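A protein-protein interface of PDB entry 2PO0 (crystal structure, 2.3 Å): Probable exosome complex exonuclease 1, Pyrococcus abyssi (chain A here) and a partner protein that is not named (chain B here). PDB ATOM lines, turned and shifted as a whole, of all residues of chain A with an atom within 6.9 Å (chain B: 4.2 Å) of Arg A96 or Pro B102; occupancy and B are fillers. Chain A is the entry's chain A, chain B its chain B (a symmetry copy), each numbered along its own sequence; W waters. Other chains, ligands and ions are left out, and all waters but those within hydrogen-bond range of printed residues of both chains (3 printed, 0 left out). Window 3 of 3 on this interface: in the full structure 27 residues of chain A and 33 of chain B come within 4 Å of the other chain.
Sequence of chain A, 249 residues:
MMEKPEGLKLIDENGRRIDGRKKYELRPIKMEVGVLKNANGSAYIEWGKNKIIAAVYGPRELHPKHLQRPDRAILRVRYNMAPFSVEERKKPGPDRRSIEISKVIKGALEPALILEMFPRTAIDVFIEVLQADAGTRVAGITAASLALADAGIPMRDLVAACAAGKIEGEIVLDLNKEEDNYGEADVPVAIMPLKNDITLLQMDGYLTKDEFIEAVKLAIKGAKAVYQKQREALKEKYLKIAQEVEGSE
NH2 of Arg A96 is in hydrogen-bond range of O of Thr B85 (3.4 Å). The guanidinium group (NH1) of Arg A96 sits close to the side-chain amide nitrogen (ND2) of Asn B86 (3.4 Å). OE1 of Glu A100 is in salt-bridge range of NH2 of Arg B111 (2.7 Å).
NH1 of Arg A96 touches CG of Pro B102, 3.8 Å away. Ile B107 touches Arg A96 (CG2 to O, 3.4 Å). Arg A96 touches Ala B110 (NH2 to CB, 3.1 Å). Arg B111 touches Arg A96. Arg A97 touches Arg B111 (CB to NH1, 3.5 Å). Ile A99 touches Ile B107.
Of the printed residues of chain B, Arg A96 touches Thr B85, Asn B86, Pro B102, Ile B107, Ala B110 and Arg B111. Pro B102 touches just one residue of chain A: Arg A96. Of the printed residues of chain B, Glu A100 touches Arg B111. Of the printed residues of chain B, Arg A97 touches Arg B111. Of the printed residues of chain A, Asn B86 touches Arg A96 (3.4 Å). Printed residues of chain A within 4 Å of Ile B107: Arg A96 and Ile A99. The nearest printed residue of chain B that does not touch Arg A96 is Ala B106 (4.7 Å). The nearest residue of chain A that does not touch Pro B102 is Ile A99 (6.0 Å). The nearest printed residue of chain A that does not touch Thr B85 is Arg A97 (10.3 Å).
Of the 8 printed residues of chain A, 4 touch a printed residue of chain B. Hydrophobic or aromatic side chains of chain A within 4 Å of the printed part of chain B: Ile A99. Printed residues of chain B that touch a printed residue of chain A: Thr B85, Asn B86, Pro B102, Ile B107, Ala B110 and Arg B111. Hydrophobic or aromatic side chains of chain B that line the printed part of chain A: Pro B102, Ile B107 and Ala B110. Among the printed residues, 9 pairs touch across the chains. Among the printed residues, Asp or Glu carboxylates within 4 Å of a Lys or Arg side-chain nitrogen of the other chain: Glu A100 with Arg B111 (2.7 Å).
Water W2 lies within hydrogen-bond range of the guanidinium group (NH2) of Arg A96 (2.6 Å), the backbone carbonyl oxygen (O) of Ala B106 (3.0 Å) and the side-chain amide nitrogen (ND2) of Asn B86 (3.4 Å). Water W1 bridges the backbone carbonyl oxygen (O) of Thr B85 (2.9 Å) and the guanidinium group (NH2) of Arg A96 (3.4 Å). Water W3 bridges the backbone carbonyl oxygen (O) of Thr B85 (3.2 Å) and the guanidinium group (NE) of Arg A96 (3.4 Å).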
ATOM      1  N   PRO A  94       9.957 -21.491   1.685  1.00  0.00           N
ATOM      2  CA  PRO A  94      10.559 -21.577   0.352  1.00  0.00           C
ATOM      3  C   PRO A  94      10.475 -23.004  -0.214  1.00  0.00           C
ATOM      4  O   PRO A  94      10.505 -23.995   0.515  1.00  0.00           O
ATOM      5  CB  PRO A  94      12.047 -21.184   0.586  1.00  0.00           C
ATOM      6  CG  PRO A  94      12.255 -21.252   2.168  1.00  0.00           C
ATOM      7  CD  PRO A  94      10.854 -20.780   2.642  1.00  0.00           C
ATOM      8  N   ASP A  95      10.329 -23.042  -1.519  1.00  0.00           N
ATOM      9  CA  ASP A  95      10.483 -24.228  -2.260  1.00  0.00           C
ATOM     10  C   ASP A  95      11.533 -23.912  -3.301  1.00  0.00           C
ATOM     11  O   ASP A  95      12.008 -22.786  -3.370  1.00  0.00           O
ATOM     12  CB  ASP A  95       9.120 -24.678  -2.877  1.00  0.00           C
ATOM     13  CG  ASP A  95       8.408 -23.595  -3.700  1.00  0.00           C
ATOM     14  OD1 ASP A  95       7.294 -23.901  -4.152  1.00  0.00           O
ATOM     15  OD2 ASP A  95       8.856 -22.459  -3.895  1.00  0.00           O
ATOM     16  N   ARG A  96      11.855 -24.900  -4.111  1.00  0.00           N
ATOM     17  CA  ARG A  96      12.856 -24.786  -5.139  1.00  0.00           C
ATOM     18  C   ARG A  96      12.534 -23.670  -6.075  1.00  0.00           C
ATOM     19  O   ARG A  96      13.394 -22.833  -6.335  1.00  0.00           O
ATOM     20  CB  ARG A  96      13.060 -26.132  -5.841  1.00  0.00           C
ATOM     21  CG  ARG A  96      13.678 -27.167  -4.913  1.00  0.00           C
ATOM     22  CD  ARG A  96      13.704 -28.507  -5.508  1.00  0.00           C
ATOM     23  NE  ARG A  96      14.701 -28.639  -6.573  1.00  0.00           N
ATOM     24  CZ  ARG A  96      15.961 -29.073  -6.400  1.00  0.00           C
ATOM     25  NH1 ARG A  96      16.402 -29.355  -5.185  1.00  0.00           N
ATOM     26  NH2 ARG A  96      16.786 -29.174  -7.427  1.00  0.00           N
ATOM     27  N   ARG A  97      11.284 -23.574  -6.518  1.00  0.00           N
ATOM     28  CA  ARG A  97      10.892 -22.462  -7.351  1.00  0.00           C
ATOM     29  C   ARG A  97      11.249 -21.108  -6.701  1.00  0.00           C
ATOM     30  O   ARG A  97      11.945 -20.346  -7.273  1.00  0.00           O
ATOM     31  CB  ARG A  97       9.389 -22.498  -7.718  1.00  0.00           C
ATOM     32  CG  ARG A  97       9.075 -21.676  -8.970  1.00  0.00           C
ATOM     33  CD  ARG A  97       7.558 -21.489  -9.362  1.00  0.00           C
ATOM     34  NE  ARG A  97       6.921 -20.586  -8.390  1.00  0.00           N
ATOM     35  CZ  ARG A  97       6.419 -19.374  -8.641  1.00  0.00           C
ATOM     36  NH1 ARG A  97       5.940 -18.693  -7.626  1.00  0.00           N
ATOM     37  NH2 ARG A  97       6.406 -18.831  -9.846  1.00  0.00           N
ATOM     38  N   SER A  98      10.696 -20.809  -5.535  1.00  0.00           N
ATOM     39  CA  SER A  98      10.967 -19.564  -4.815  1.00  0.00           C
ATOM     40  C   SER A  98      12.459 -19.267  -4.632  1.00  0.00           C
ATOM     41  O   SER A  98      12.827 -18.123  -4.592  1.00  0.00           O
ATOM     42  CB  SER A  98      10.368 -19.688  -3.429  1.00  0.00           C
ATOM     43  OG  SER A  98       8.960 -19.689  -3.563  1.00  0.00           O
ATOM     44  N   ILE A  99      13.281 -20.314  -4.455  1.00  0.00           N
ATOM     45  CA  ILE A  99      14.696 -20.147  -4.181  1.00  0.00           C
ATOM     46  C   ILE A  99      15.298 -19.561  -5.434  1.00  0.00           C
ATOM     47  O   ILE A  99      16.076 -18.607  -5.358  1.00  0.00           O
ATOM     48  CB  ILE A  99      15.403 -21.449  -3.814  1.00  0.00           C
ATOM     49  CG1 ILE A  99      14.848 -22.071  -2.507  1.00  0.00           C
ATOM     50  CG2 ILE A  99      16.888 -21.265  -3.760  1.00  0.00           C
ATOM     51  CD1 ILE A  99      14.874 -21.292  -1.424  1.00  0.00           C
ATOM     52  N   GLU A 100      14.882 -20.124  -6.581  1.00  0.00           N
ATOM     53  CA  GLU A 100      15.404 -19.769  -7.877  1.00  0.00           C
ATOM     54  C   GLU A 100      15.008 -18.341  -8.285  1.00  0.00           C
ATOM     55  O   GLU A 100      15.808 -17.611  -8.852  1.00  0.00           O
ATOM     56  CB  GLU A 100      15.003 -20.778  -8.967  1.00  0.00           C
ATOM     57  CG  GLU A 100      15.555 -20.320 -10.393  1.00  0.00           C
ATOM     58  CD  GLU A 100      14.878 -20.882 -11.664  1.00  0.00           C
ATOM     59  OE1 GLU A 100      13.885 -21.612 -11.600  1.00  0.00           O
ATOM     60  OE2 GLU A 100      15.346 -20.547 -12.769  1.00  0.00           O
ATOM     61  N   ILE A 101      13.760 -17.977  -8.037  1.00  0.00           N
ATOM     62  CA  ILE A 101      13.266 -16.672  -8.345  1.00  0.00           C
ATOM     63  C   ILE A 101      13.944 -15.611  -7.482  1.00  0.00           C
ATOM     64  O   ILE A 101      14.340 -14.580  -7.964  1.00  0.00           O
ATOM     65  CB  ILE A 101      11.734 -16.605  -8.188  1.00  0.00           C
ATOM     66  CG1 ILE A 101      11.034 -17.650  -9.088  1.00  0.00           C
ATOM     67  CG2 ILE A 101      11.239 -15.169  -8.366  1.00  0.00           C
ATOM     68  CD1 ILE A 101       9.460 -17.603  -8.984  1.00  0.00           C
ATOM     69  N   THR B  85      15.211 -33.940 -11.142  1.00  0.00           N
ATOM     70  CA  THR B  85      16.637 -33.520 -11.282  1.00  0.00           C
ATOM     71  C   THR B  85      17.131 -32.839 -10.003  1.00  0.00           C
ATOM     72  O   THR B  85      16.516 -31.936  -9.450  1.00  0.00           O
ATOM     73  CB  THR B  85      16.896 -32.563 -12.499  1.00  0.00           C
ATOM     74  OG1 THR B  85      16.206 -33.040 -13.671  1.00  0.00           O
ATOM     75  CG2 THR B  85      18.423 -32.441 -12.800  1.00  0.00           C
ATOM     76  N   ASN B  86      18.226 -33.365  -9.508  1.00  0.00           N
ATOM     77  CA  ASN B  86      18.859 -32.901  -8.313  1.00  0.00           C
ATOM     78  C   ASN B  86      20.322 -32.768  -8.613  1.00  0.00           C
ATOM     79  O   ASN B  86      20.905 -33.632  -9.242  1.00  0.00           O
ATOM     80  CB  ASN B  86      18.681 -33.859  -7.133  1.00  0.00           C
ATOM     81  CG  ASN B  86      19.067 -33.193  -5.849  1.00  0.00           C
ATOM     82  OD1 ASN B  86      20.054 -33.549  -5.159  1.00  0.00           O
ATOM     83  ND2 ASN B  86      18.354 -32.142  -5.552  1.00  0.00           N
ATOM     84  N   GLY B 100      25.290 -29.515   3.370  1.00  0.00           N
ATOM     85  CA  GLY B 100      23.833 -29.260   3.667  1.00  0.00           C
ATOM     86  C   GLY B 100      22.910 -29.336   2.429  1.00  0.00           C
ATOM     87  O   GLY B 100      23.372 -29.728   1.293  1.00  0.00           O
ATOM     88  N   PRO B 101      21.599 -28.979   2.601  1.00  0.00           N
ATOM     89  CA  PRO B 101      20.582 -29.030   1.495  1.00  0.00           C
ATOM     90  C   PRO B 101      20.951 -28.121   0.327  1.00  0.00           C
ATOM     91  O   PRO B 101      21.709 -27.154   0.594  1.00  0.00           O
ATOM     92  CB  PRO B 101      19.296 -28.516   2.182  1.00  0.00           C
ATOM     93  CG  PRO B 101      19.760 -27.787   3.422  1.00  0.00           C
ATOM     94  CD  PRO B 101      20.986 -28.567   3.881  1.00  0.00           C
ATOM     95  N   PRO B 102      20.433 -28.373  -0.933  1.00  0.00           N
ATOM     96  CA  PRO B 102      20.914 -27.548  -2.050  1.00  0.00           C
ATOM     97  C   PRO B 102      20.927 -26.069  -1.692  1.00  0.00           C
ATOM     98  O   PRO B 102      20.010 -25.595  -0.984  1.00  0.00           O
ATOM     99  CB  PRO B 102      19.881 -27.798  -3.167  1.00  0.00           C
ATOM    100  CG  PRO B 102      19.549 -29.199  -3.048  1.00  0.00           C
ATOM    101  CD  PRO B 102      19.450 -29.370  -1.439  1.00  0.00           C
ATOM    102  N   ASP B 103      21.949 -25.324  -2.099  1.00  0.00           N
ATOM    103  CA  ASP B 103      21.796 -23.922  -1.889  1.00  0.00           C
ATOM    104  C   ASP B 103      21.114 -23.483  -3.172  1.00  0.00           C
ATOM    105  O   ASP B 103      20.710 -24.317  -3.967  1.00  0.00           O
ATOM    106  CB  ASP B 103      23.141 -23.254  -1.654  1.00  0.00           C
ATOM    107  CG  ASP B 103      23.996 -23.208  -2.904  1.00  0.00           C
ATOM    108  OD1 ASP B 103      24.107 -24.256  -3.635  1.00  0.00           O
ATOM    109  OD2 ASP B 103      24.565 -22.094  -3.134  1.00  0.00           O
ATOM    110  N   ALA B 106      22.674 -24.773  -6.332  1.00  0.00           N
ATOM    111  CA  ALA B 106      22.436 -26.163  -6.680  1.00  0.00           C
ATOM    112  C   ALA B 106      21.043 -26.212  -7.214  1.00  0.00           C
ATOM    113  O   ALA B 106      20.809 -26.881  -8.134  1.00  0.00           O
ATOM    114  CB  ALA B 106      22.566 -27.040  -5.463  1.00  0.00           C
ATOM    115  N   ILE B 107      20.118 -25.438  -6.632  1.00  0.00           N
ATOM    116  CA  ILE B 107      18.731 -25.417  -7.048  1.00  0.00           C
ATOM    117  C   ILE B 107      18.616 -24.848  -8.485  1.00  0.00           C
ATOM    118  O   ILE B 107      18.034 -25.474  -9.385  1.00  0.00           O
ATOM    119  CB  ILE B 107      17.847 -24.719  -5.924  1.00  0.00           C
ATOM    120  CG1 ILE B 107      17.721 -25.698  -4.726  1.00  0.00           C
ATOM    121  CG2 ILE B 107      16.461 -24.252  -6.493  1.00  0.00           C
ATOM    122  CD1 ILE B 107      17.269 -25.141  -3.532  1.00  0.00           C
ATOM    123  N   ALA B 110      20.019 -27.252 -11.093  1.00  0.00           N
ATOM    124  CA  ALA B 110      19.101 -28.384 -11.245  1.00  0.00           C
ATOM    125  C   ALA B 110      17.883 -28.042 -12.110  1.00  0.00           C
ATOM    126  O   ALA B 110      17.539 -28.777 -13.027  1.00  0.00           O
ATOM    127  CB  ALA B 110      18.647 -28.967  -9.851  1.00  0.00           C
ATOM    128  N   ARG B 111      17.296 -26.882 -11.825  1.00  0.00           N
ATOM    129  CA  ARG B 111      16.071 -26.432 -12.399  1.00  0.00           C
ATOM    130  C   ARG B 111      16.178 -26.064 -13.853  1.00  0.00           C
ATOM    131  O   ARG B 111      15.305 -26.401 -14.599  1.00  0.00           O
ATOM    132  CB  ARG B 111      15.534 -25.241 -11.618  1.00  0.00           C
ATOM    133  CG  ARG B 111      14.762 -25.579 -10.409  1.00  0.00           C
ATOM    134  CD  ARG B 111      14.002 -24.287  -9.888  1.00  0.00           C
ATOM    135  NE  ARG B 111      12.618 -24.682  -9.775  1.00  0.00           N
ATOM    136  CZ  ARG B 111      11.580 -24.194 -10.427  1.00  0.00           C
ATOM    137  NH1 ARG B 111      10.433 -24.742 -10.205  1.00  0.00           N
ATOM    138  NH2 ARG B 111      11.667 -23.182 -11.252  1.00  0.00           N
HETATM  139  O   HOH W   1      14.970 -29.568 -10.245  1.00  0.00           O
HETATM  140  O   HOH W   2      19.306 -29.241  -6.951  1.00  0.00           O
HETATM  141  O   HOH W   3      14.712 -32.012  -6.823  1.00  0.00           O
